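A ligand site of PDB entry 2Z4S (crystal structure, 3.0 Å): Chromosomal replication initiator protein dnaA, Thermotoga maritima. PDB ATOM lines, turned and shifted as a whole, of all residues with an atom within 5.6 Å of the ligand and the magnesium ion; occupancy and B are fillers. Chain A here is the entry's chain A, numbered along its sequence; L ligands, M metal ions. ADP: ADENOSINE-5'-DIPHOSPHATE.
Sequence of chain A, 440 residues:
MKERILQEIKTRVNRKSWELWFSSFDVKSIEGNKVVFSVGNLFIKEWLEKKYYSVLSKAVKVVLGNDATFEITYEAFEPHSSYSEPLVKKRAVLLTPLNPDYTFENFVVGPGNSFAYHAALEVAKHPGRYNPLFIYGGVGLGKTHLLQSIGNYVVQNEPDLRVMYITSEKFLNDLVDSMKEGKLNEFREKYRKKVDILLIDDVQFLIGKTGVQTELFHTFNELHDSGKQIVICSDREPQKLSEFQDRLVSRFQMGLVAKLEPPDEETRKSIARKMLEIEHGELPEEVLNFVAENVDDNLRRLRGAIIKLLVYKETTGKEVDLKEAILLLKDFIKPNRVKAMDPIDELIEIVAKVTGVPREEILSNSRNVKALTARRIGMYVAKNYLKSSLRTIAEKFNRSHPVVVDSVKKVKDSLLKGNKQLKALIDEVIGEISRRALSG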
ATOM      1  N   ASP A 101     -10.819 -12.648 -29.277  1.00  0.00           N
ATOM      2  CA  ASP A 101      -9.494 -12.120 -29.572  1.00  0.00           C
ATOM      3  C   ASP A 101      -8.455 -12.622 -28.586  1.00  0.00           C
ATOM      4  O   ASP A 101      -7.325 -12.934 -28.960  1.00  0.00           O
ATOM      5  CB  ASP A 101      -9.499 -10.602 -29.550  1.00  0.00           C
ATOM      6  CG  ASP A 101     -10.396 -10.015 -30.605  1.00  0.00           C
ATOM      7  OD1 ASP A 101     -10.861 -10.789 -31.480  1.00  0.00           O
ATOM      8  OD2 ASP A 101     -10.622  -8.781 -30.568  1.00  0.00           O
ATOM      9  N   TYR A 102      -8.831 -12.689 -27.312  1.00  0.00           N
ATOM     10  CA  TYR A 102      -7.933 -13.133 -26.255  1.00  0.00           C
ATOM     11  C   TYR A 102      -7.613 -14.606 -26.307  1.00  0.00           C
ATOM     12  O   TYR A 102      -8.213 -15.423 -25.614  1.00  0.00           O
ATOM     13  CB  TYR A 102      -8.547 -12.786 -24.905  1.00  0.00           C
ATOM     14  CG  TYR A 102      -8.732 -11.305 -24.723  1.00  0.00           C
ATOM     15  CD1 TYR A 102      -9.603 -10.801 -23.765  1.00  0.00           C
ATOM     16  CD2 TYR A 102      -8.033 -10.407 -25.532  1.00  0.00           C
ATOM     17  CE1 TYR A 102      -9.773  -9.432 -23.608  1.00  0.00           C
ATOM     18  CE2 TYR A 102      -8.195  -9.057 -25.384  1.00  0.00           C
ATOM     19  CZ  TYR A 102      -9.065  -8.570 -24.422  1.00  0.00           C
ATOM     20  OH  TYR A 102      -9.181  -7.207 -24.289  1.00  0.00           O
ATOM     21  N   ASN A 106      -3.207 -15.051 -30.549  1.00  0.00           N
ATOM     22  CA  ASN A 106      -3.099 -13.635 -30.871  1.00  0.00           C
ATOM     23  C   ASN A 106      -2.152 -12.937 -29.919  1.00  0.00           C
ATOM     24  O   ASN A 106      -2.113 -11.706 -29.843  1.00  0.00           O
ATOM     25  CB  ASN A 106      -4.458 -12.963 -30.826  1.00  0.00           C
ATOM     26  CG  ASN A 106      -5.451 -13.658 -31.704  1.00  0.00           C
ATOM     27  OD1 ASN A 106      -5.082 -14.228 -32.727  1.00  0.00           O
ATOM     28  ND2 ASN A 106      -6.716 -13.616 -31.314  1.00  0.00           N
ATOM     29  N   PHE A 107      -1.371 -13.727 -29.195  1.00  0.00           N
ATOM     30  CA  PHE A 107      -0.433 -13.162 -28.250  1.00  0.00           C
ATOM     31  C   PHE A 107       0.978 -13.293 -28.788  1.00  0.00           C
ATOM     32  O   PHE A 107       1.507 -14.380 -28.943  1.00  0.00           O
ATOM     33  CB  PHE A 107      -0.542 -13.867 -26.894  1.00  0.00           C
ATOM     34  CG  PHE A 107       0.074 -13.086 -25.750  1.00  0.00           C
ATOM     35  CD1 PHE A 107      -0.687 -12.202 -25.011  1.00  0.00           C
ATOM     36  CD2 PHE A 107       1.426 -13.214 -25.459  1.00  0.00           C
ATOM     37  CE1 PHE A 107      -0.110 -11.459 -23.984  1.00  0.00           C
ATOM     38  CE2 PHE A 107       2.009 -12.474 -24.445  1.00  0.00           C
ATOM     39  CZ  PHE A 107       1.234 -11.590 -23.703  1.00  0.00           C
ATOM     40  N   VAL A 108       1.553 -12.142 -29.094  1.00  0.00           N
ATOM     41  CA  VAL A 108       2.910 -12.053 -29.590  1.00  0.00           C
ATOM     42  C   VAL A 108       3.863 -12.135 -28.391  1.00  0.00           C
ATOM     43  O   VAL A 108       3.757 -11.354 -27.452  1.00  0.00           O
ATOM     44  CB  VAL A 108       3.099 -10.695 -30.311  1.00  0.00           C
ATOM     45  CG1 VAL A 108       4.554 -10.446 -30.598  1.00  0.00           C
ATOM     46  CG2 VAL A 108       2.268 -10.695 -31.576  1.00  0.00           C
ATOM     47  N   VAL A 109       4.806 -13.076 -28.432  1.00  0.00           N
ATOM     48  CA  VAL A 109       5.754 -13.218 -27.332  1.00  0.00           C
ATOM     49  C   VAL A 109       6.990 -12.339 -27.494  1.00  0.00           C
ATOM     50  O   VAL A 109       7.349 -11.954 -28.608  1.00  0.00           O
ATOM     51  CB  VAL A 109       6.200 -14.674 -27.181  1.00  0.00           C
ATOM     52  CG1 VAL A 109       7.125 -14.798 -25.992  1.00  0.00           C
ATOM     53  CG2 VAL A 109       4.983 -15.551 -26.988  1.00  0.00           C
ATOM     54  N   ASN A 113       7.230 -10.471 -21.937  1.00  0.00           N
ATOM     55  CA  ASN A 113       6.012 -11.167 -21.564  1.00  0.00           C
ATOM     56  C   ASN A 113       6.054 -12.658 -21.833  1.00  0.00           C
ATOM     57  O   ASN A 113       5.028 -13.328 -21.768  1.00  0.00           O
ATOM     58  CB  ASN A 113       4.829 -10.584 -22.306  1.00  0.00           C
ATOM     59  CG  ASN A 113       4.883 -10.836 -23.800  1.00  0.00           C
ATOM     60  OD1 ASN A 113       4.034 -10.375 -24.554  1.00  0.00           O
ATOM     61  ND2 ASN A 113       5.895 -11.565 -24.230  1.00  0.00           N
ATOM     62  N   GLY A 137       1.122  -7.056 -13.595  1.00  0.00           N
ATOM     63  CA  GLY A 137       1.855  -6.107 -14.401  1.00  0.00           C
ATOM     64  C   GLY A 137       1.040  -4.845 -14.583  1.00  0.00           C
ATOM     65  O   GLY A 137      -0.160  -4.842 -14.330  1.00  0.00           O
ATOM     66  N   GLY A 138       1.695  -3.772 -15.043  1.00  0.00           N
ATOM     67  CA  GLY A 138       1.019  -2.504 -15.248  1.00  0.00           C
ATOM     68  C   GLY A 138      -0.171  -2.581 -16.184  1.00  0.00           C
ATOM     69  O   GLY A 138      -0.543  -3.655 -16.627  1.00  0.00           O
ATOM     70  N   VAL A 139      -0.758  -1.439 -16.498  1.00  0.00           N
ATOM     71  CA  VAL A 139      -1.924  -1.420 -17.390  1.00  0.00           C
ATOM     72  C   VAL A 139      -1.540  -1.760 -18.826  1.00  0.00           C
ATOM     73  O   VAL A 139      -0.404  -1.528 -19.270  1.00  0.00           O
ATOM     74  CB  VAL A 139      -2.601  -0.059 -17.405  1.00  0.00           C
ATOM     75  CG1 VAL A 139      -4.076  -0.253 -17.353  1.00  0.00           C
ATOM     76  CG2 VAL A 139      -2.115   0.778 -16.247  1.00  0.00           C
ATOM     77  N   GLY A 140      -2.515  -2.304 -19.550  1.00  0.00           N
ATOM     78  CA  GLY A 140      -2.299  -2.686 -20.928  1.00  0.00           C
ATOM     79  C   GLY A 140      -1.005  -3.437 -21.178  1.00  0.00           C
ATOM     80  O   GLY A 140      -0.142  -2.943 -21.893  1.00  0.00           O
ATOM     81  N   LEU A 141      -0.852  -4.625 -20.595  1.00  0.00           N
ATOM     82  CA  LEU A 141       0.347  -5.388 -20.810  1.00  0.00           C
ATOM     83  C   LEU A 141       0.050  -6.857 -21.041  1.00  0.00           C
ATOM     84  O   LEU A 141       0.965  -7.677 -21.041  1.00  0.00           O
ATOM     85  CB  LEU A 141       1.299  -5.259 -19.646  1.00  0.00           C
ATOM     86  CG  LEU A 141       1.817  -3.885 -19.276  1.00  0.00           C
ATOM     87  CD1 LEU A 141       2.970  -4.081 -18.299  1.00  0.00           C
ATOM     88  CD2 LEU A 141       2.299  -3.128 -20.493  1.00  0.00           C
ATOM     89  N   GLY A 142      -1.221  -7.202 -21.195  1.00  0.00           N
ATOM     90  CA  GLY A 142      -1.541  -8.584 -21.453  1.00  0.00           C
ATOM     91  C   GLY A 142      -2.262  -9.396 -20.399  1.00  0.00           C
ATOM     92  O   GLY A 142      -2.673 -10.538 -20.665  1.00  0.00           O
ATOM     93  N   LYS A 143      -2.445  -8.835 -19.206  1.00  0.00           N
ATOM     94  CA  LYS A 143      -3.120  -9.543 -18.108  1.00  0.00           C
ATOM     95  C   LYS A 143      -4.496 -10.110 -18.483  1.00  0.00           C
ATOM     96  O   LYS A 143      -4.728 -11.313 -18.370  1.00  0.00           O
ATOM     97  CB  LYS A 143      -3.266  -8.634 -16.893  1.00  0.00           C
ATOM     98  CG  LYS A 143      -1.983  -7.986 -16.447  1.00  0.00           C
ATOM     99  CD  LYS A 143      -2.124  -7.390 -15.074  1.00  0.00           C
ATOM    100  CE  LYS A 143      -3.022  -6.195 -15.082  1.00  0.00           C
ATOM    101  NZ  LYS A 143      -2.267  -5.070 -15.659  1.00  0.00           N
ATOM    102  N   THR A 144      -5.406  -9.260 -18.930  1.00  0.00           N
ATOM    103  CA  THR A 144      -6.723  -9.763 -19.280  1.00  0.00           C
ATOM    104  C   THR A 144      -6.626 -10.753 -20.420  1.00  0.00           C
ATOM    105  O   THR A 144      -7.212 -11.838 -20.380  1.00  0.00           O
ATOM    106  CB  THR A 144      -7.669  -8.643 -19.734  1.00  0.00           C
ATOM    107  OG1 THR A 144      -7.778  -7.649 -18.700  1.00  0.00           O
ATOM    108  CG2 THR A 144      -9.028  -9.226 -20.053  1.00  0.00           C
ATOM    109  N   HIS A 145      -5.863 -10.369 -21.432  1.00  0.00           N
ATOM    110  CA  HIS A 145      -5.695 -11.178 -22.611  1.00  0.00           C
ATOM    111  C   HIS A 145      -5.125 -12.548 -22.297  1.00  0.00           C
ATOM    112  O   HIS A 145      -5.599 -13.560 -22.816  1.00  0.00           O
ATOM    113  CB  HIS A 145      -4.817 -10.426 -23.598  1.00  0.00           C
ATOM    114  CG  HIS A 145      -4.655 -11.113 -24.913  1.00  0.00           C
ATOM    115  ND1 HIS A 145      -4.285 -10.447 -26.048  1.00  0.00           N
ATOM    116  CD2 HIS A 145      -4.777 -12.421 -25.254  1.00  0.00           C
ATOM    117  CE1 HIS A 145      -4.185 -11.309 -27.050  1.00  0.00           C
ATOM    118  NE2 HIS A 145      -4.474 -12.511 -26.588  1.00  0.00           N
ATOM    119  N   LEU A 146      -4.109 -12.591 -21.453  1.00  0.00           N
ATOM    120  CA  LEU A 146      -3.479 -13.848 -21.082  1.00  0.00           C
ATOM    121  C   LEU A 146      -4.469 -14.691 -20.285  1.00  0.00           C
ATOM    122  O   LEU A 146      -4.678 -15.868 -20.548  1.00  0.00           O
ATOM    123  CB  LEU A 146      -2.223 -13.570 -20.253  1.00  0.00           C
ATOM    124  CG  LEU A 146      -0.890 -14.242 -20.588  1.00  0.00           C
ATOM    125  CD1 LEU A 146      -0.825 -14.624 -22.059  1.00  0.00           C
ATOM    126  CD2 LEU A 146       0.259 -13.283 -20.213  1.00  0.00           C
ATOM    127  N   ASP A 201     -10.027 -11.517 -12.727  1.00  0.00           N
ATOM    128  CA  ASP A 201      -9.280 -10.377 -13.264  1.00  0.00           C
ATOM    129  C   ASP A 201      -9.215  -9.199 -12.299  1.00  0.00           C
ATOM    130  O   ASP A 201     -10.014  -9.095 -11.370  1.00  0.00           O
ATOM    131  CB  ASP A 201      -9.899  -9.918 -14.584  1.00  0.00           C
ATOM    132  CG  ASP A 201      -8.856  -9.511 -15.628  1.00  0.00           C
ATOM    133  OD1 ASP A 201      -7.792  -8.939 -15.270  1.00  0.00           O
ATOM    134  OD2 ASP A 201      -9.120  -9.743 -16.828  1.00  0.00           O
ATOM    135  N   ASP A 202      -8.258  -8.305 -12.546  1.00  0.00           N
ATOM    136  CA  ASP A 202      -8.048  -7.111 -11.743  1.00  0.00           C
ATOM    137  C   ASP A 202      -8.450  -7.273 -10.305  1.00  0.00           C
ATOM    138  O   ASP A 202      -9.555  -6.900  -9.934  1.00  0.00           O
ATOM    139  CB  ASP A 202      -8.810  -5.936 -12.328  1.00  0.00           C
ATOM    140  CG  ASP A 202      -8.321  -5.559 -13.698  1.00  0.00           C
ATOM    141  OD1 ASP A 202      -7.259  -4.903 -13.808  1.00  0.00           O
ATOM    142  OD2 ASP A 202      -8.994  -5.941 -14.674  1.00  0.00           O
ATOM    143  N   LEU A 260       4.439  -9.400 -16.065  1.00  0.00           N
ATOM    144  CA  LEU A 260       4.473  -8.867 -17.409  1.00  0.00           C
ATOM    145  C   LEU A 260       5.189  -7.526 -17.371  1.00  0.00           C
ATOM    146  O   LEU A 260       5.052  -6.777 -16.407  1.00  0.00           O
ATOM    147  CB  LEU A 260       3.055  -8.665 -17.942  1.00  0.00           C
ATOM    148  CG  LEU A 260       2.250  -9.917 -18.322  1.00  0.00           C
ATOM    149  CD1 LEU A 260       0.792  -9.582 -18.457  1.00  0.00           C
ATOM    150  CD2 LEU A 260       2.744 -10.467 -19.632  1.00  0.00           C
ATOM    151  N   ILE A 271       3.313  -6.724 -32.392  1.00  0.00           N
ATOM    152  CA  ILE A 271       2.017  -6.737 -31.724  1.00  0.00           C
ATOM    153  C   ILE A 271       1.081  -5.857 -32.536  1.00  0.00           C
ATOM    154  O   ILE A 271      -0.071  -6.216 -32.794  1.00  0.00           O
ATOM    155  CB  ILE A 271       2.133  -6.186 -30.285  1.00  0.00           C
ATOM    156  CG1 ILE A 271       2.905  -7.185 -29.413  1.00  0.00           C
ATOM    157  CG2 ILE A 271       0.738  -5.936 -29.702  1.00  0.00           C
ATOM    158  CD1 ILE A 271       3.128  -6.709 -28.001  1.00  0.00           C
ATOM    159  N   LYS A 274      -0.139  -7.733 -35.452  1.00  0.00           N
ATOM    160  CA  LYS A 274      -1.091  -8.754 -35.038  1.00  0.00           C
ATOM    161  C   LYS A 274      -2.411  -8.129 -34.680  1.00  0.00           C
ATOM    162  O   LYS A 274      -3.462  -8.733 -34.879  1.00  0.00           O
ATOM    163  CB  LYS A 274      -0.576  -9.530 -33.835  1.00  0.00           C
ATOM    164  CG  LYS A 274      -1.413 -10.757 -33.479  1.00  0.00           C
ATOM    165  CD  LYS A 274      -1.271 -11.843 -34.511  1.00  0.00           C
ATOM    166  CE  LYS A 274      -2.044 -13.086 -34.119  1.00  0.00           C
ATOM    167  NZ  LYS A 274      -2.046 -14.134 -35.186  1.00  0.00           N
ATOM    168  N   MET A 275      -2.362  -6.923 -34.115  1.00  0.00           N
ATOM    169  CA  MET A 275      -3.583  -6.214 -33.743  1.00  0.00           C
ATOM    170  C   MET A 275      -4.370  -5.941 -35.007  1.00  0.00           C
ATOM    171  O   MET A 275      -5.582  -6.137 -35.059  1.00  0.00           O
ATOM    172  CB  MET A 275      -3.239  -4.925 -33.014  1.00  0.00           C
ATOM    173  CG  MET A 275      -3.500  -4.983 -31.517  1.00  0.00           C
ATOM    174  SD  MET A 275      -2.440  -3.876 -30.587  1.00  0.00           S
ATOM    175  CE  MET A 275      -2.346  -2.523 -31.717  1.00  0.00           C
ATOM    176  N   LEU A 299      -0.452  -1.392 -24.289  1.00  0.00           N
ATOM    177  CA  LEU A 299      -0.930  -1.932 -25.527  1.00  0.00           C
ATOM    178  C   LEU A 299      -2.403  -1.643 -25.721  1.00  0.00           C
ATOM    179  O   LEU A 299      -2.953  -1.899 -26.790  1.00  0.00           O
ATOM    180  CB  LEU A 299      -0.640  -3.422 -25.557  1.00  0.00           C
ATOM    181  CG  LEU A 299       0.846  -3.763 -25.385  1.00  0.00           C
ATOM    182  CD1 LEU A 299       1.022  -5.246 -25.447  1.00  0.00           C
ATOM    183  CD2 LEU A 299       1.672  -3.100 -26.453  1.00  0.00           C
ATOM    184  N   ARG A 300      -3.053  -1.088 -24.707  1.00  0.00           N
ATOM    185  CA  ARG A 300      -4.482  -0.769 -24.843  1.00  0.00           C
ATOM    186  C   ARG A 300      -4.593   0.434 -25.777  1.00  0.00           C
ATOM    187  O   ARG A 300      -5.438   0.473 -26.676  1.00  0.00           O
ATOM    188  CB  ARG A 300      -5.116  -0.430 -23.492  1.00  0.00           C
ATOM    189  CG  ARG A 300      -6.632  -0.466 -23.513  1.00  0.00           C
ATOM    190  CD  ARG A 300      -7.272   0.543 -22.572  1.00  0.00           C
ATOM    191  NE  ARG A 300      -6.759   0.486 -21.206  1.00  0.00           N
ATOM    192  CZ  ARG A 300      -6.716  -0.614 -20.437  1.00  0.00           C
ATOM    193  NH1 ARG A 300      -7.150  -1.780 -20.894  1.00  0.00           N
ATOM    194  NH2 ARG A 300      -6.245  -0.541 -19.207  1.00  0.00           N
ATOM    195  N   ARG A 303      -3.354  -0.186 -29.519  1.00  0.00           N
ATOM    196  CA  ARG A 303      -4.442  -0.715 -30.315  1.00  0.00           C
ATOM    197  C   ARG A 303      -5.458   0.373 -30.550  1.00  0.00           C
ATOM    198  O   ARG A 303      -6.053   0.466 -31.615  1.00  0.00           O
ATOM    199  CB  ARG A 303      -5.107  -1.876 -29.593  1.00  0.00           C
ATOM    200  CG  ARG A 303      -6.249  -2.472 -30.350  1.00  0.00           C
ATOM    201  CD  ARG A 303      -7.458  -2.547 -29.471  1.00  0.00           C
ATOM    202  NE  ARG A 303      -8.524  -3.301 -30.119  1.00  0.00           N
ATOM    203  CZ  ARG A 303      -9.754  -3.401 -29.639  1.00  0.00           C
ATOM    204  NH1 ARG A 303     -10.062  -2.803 -28.497  1.00  0.00           N
ATOM    205  NH2 ARG A 303     -10.674  -4.102 -30.293  1.00  0.00           N
HETATM  206  PB  ADP L   1      -4.274  -5.259 -19.205  1.00  0.00           P
HETATM  207  O1B ADP L   1      -3.565  -6.524 -18.972  1.00  0.00           O
HETATM  208  O2B ADP L   1      -3.575  -4.110 -18.367  1.00  0.00           O
HETATM  209  O3B ADP L   1      -5.819  -5.400 -18.782  1.00  0.00           O
HETATM  210  PA  ADP L   1      -4.841  -5.921 -21.718  1.00  0.00           P
HETATM  211  O1A ADP L   1      -4.221  -7.250 -21.571  1.00  0.00           O
HETATM  212  O2A ADP L   1      -6.404  -6.049 -21.406  1.00  0.00           O
HETATM  213  O3A ADP L   1      -4.165  -4.822 -20.732  1.00  0.00           O
HETATM  214  O5' ADP L   1      -4.644  -5.313 -23.183  1.00  0.00           O
HETATM  215  C5' ADP L   1      -5.203  -6.269 -24.035  1.00  0.00           C
HETATM  216  C4' ADP L   1      -5.137  -5.837 -25.469  1.00  0.00           C
HETATM  217  O4' ADP L   1      -3.786  -5.575 -25.864  1.00  0.00           O
HETATM  218  C3' ADP L   1      -5.736  -6.980 -26.269  1.00  0.00           C
HETATM  219  O3' ADP L   1      -6.888  -6.560 -27.004  1.00  0.00           O
HETATM  220  C2' ADP L   1      -4.609  -7.487 -27.155  1.00  0.00           C
HETATM  221  O2' ADP L   1      -5.004  -7.443 -28.548  1.00  0.00           O
HETATM  222  C1' ADP L   1      -3.407  -6.566 -26.859  1.00  0.00           C
HETATM  223  N9  ADP L   1      -2.214  -7.301 -26.407  1.00  0.00           N
HETATM  224  C8  ADP L   1      -1.677  -7.330 -25.154  1.00  0.00           C
HETATM  225  N7  ADP L   1      -0.619  -8.084 -25.132  1.00  0.00           N
HETATM  226  C5  ADP L   1      -0.408  -8.579 -26.359  1.00  0.00           C
HETATM  227  C6  ADP L   1       0.555  -9.428 -26.946  1.00  0.00           C
HETATM  228  N6  ADP L   1       1.600  -9.931 -26.190  1.00  0.00           N
HETATM  229  N1  ADP L   1       0.455  -9.733 -28.258  1.00  0.00           N
HETATM  230  C2  ADP L   1      -0.545  -9.249 -29.008  1.00  0.00           C
HETATM  231  N3  ADP L   1      -1.467  -8.442 -28.488  1.00  0.00           N
HETATM  232  C4  ADP L   1      -1.436  -8.093 -27.189  1.00  0.00           C
HETATM  233 MG    MG M   1      -7.136  -6.217 -16.857  1.00  0.00          MG
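The magnesium ion is bound by the side-chain hydroxyl (OG1) of Thr 144 (2.4 Å) and an oxygen (O3B) of the ligand (2.5 Å). The magnesium ion has two donor atoms within binding distance.
A nitrogen (N1) of the ligand lies within hydrogen-bond range of the backbone NH (N) of Val 108, at 2.8 Å. The backbone NH (N) of Gly 140 sits at hydrogen-bond distance from an oxygen (O2B) of the ligand, 2.4 Å away. The backbone NH of Leu 141 lies within hydrogen-bond range of an oxygen (O3A) of the ligand, at 3.3 Å. N6 of the ligand is in hydrogen-bond range of OD1 of Asn 113. O of Val 108 sits at hydrogen-bond distance from N6 of the ligand (2.9 Å). N of Thr 144 is in hydrogen-bond range of O1B of the ligand (3.3 Å). An oxygen (O2B) of the ligand is in salt-bridge range of the side-chain amino group of Lys 143 (3.2 Å). O1A of the ligand lies close to N of Gly 142 (3.0 Å). N of Lys 143 lies within hydrogen-bond range of O1B of the ligand (2.6 Å).
OD1 of Asp 201 touches the magnesium ion, at 3.2 Å. OD2 of Asp 202 touches the magnesium ion, at 2.9 Å. Three residues have an atom within 4 Å of the magnesium ion: Thr 144, Asp 201 and Asp 202. The nearest printed residue that does not touch the magnesium ion is Lys 143 (4.5 Å).
Residues that only touch the ligand: Phe 107, Asn 106, Val 139, His 145, Tyr 102, Leu 299, Gly 138 and Ile 271. Hydrophobic or aromatic side chains within 4 Å of the ligand: Tyr 102, Phe 107, Val 108, His 145, Ile 271 and Leu 299. Along chain A the residues within 4 Å of the ligand span positions 102 to 299. The nearest printed residue that does not touch the ligand is Met 275 (4.1 Å).
OG1 of Thr 144 sits close to OD2 of Asp 201 (3.1 Å). NZ of Lys 143 is in hydrogen-bond range of O of Gly 137 (2.5 Å). O of Val 108 lies close to OD1 of Asn 113. The side-chain amide nitrogen (ND2) of Asn 106 sits at hydrogen-bond distance from the backbone carbonyl oxygen (O) of Asp 101, 2.5 Å away. The backbone NH (N) of Leu 299 is in hydrogen-bond range of the backbone carbonyl oxygen (O) of Gly 140 (2.9 Å). The side-chain amino group (NZ) of Lys 143 is in hydrogen-bond range of the backbone carbonyl oxygen (O) of Gly 138.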
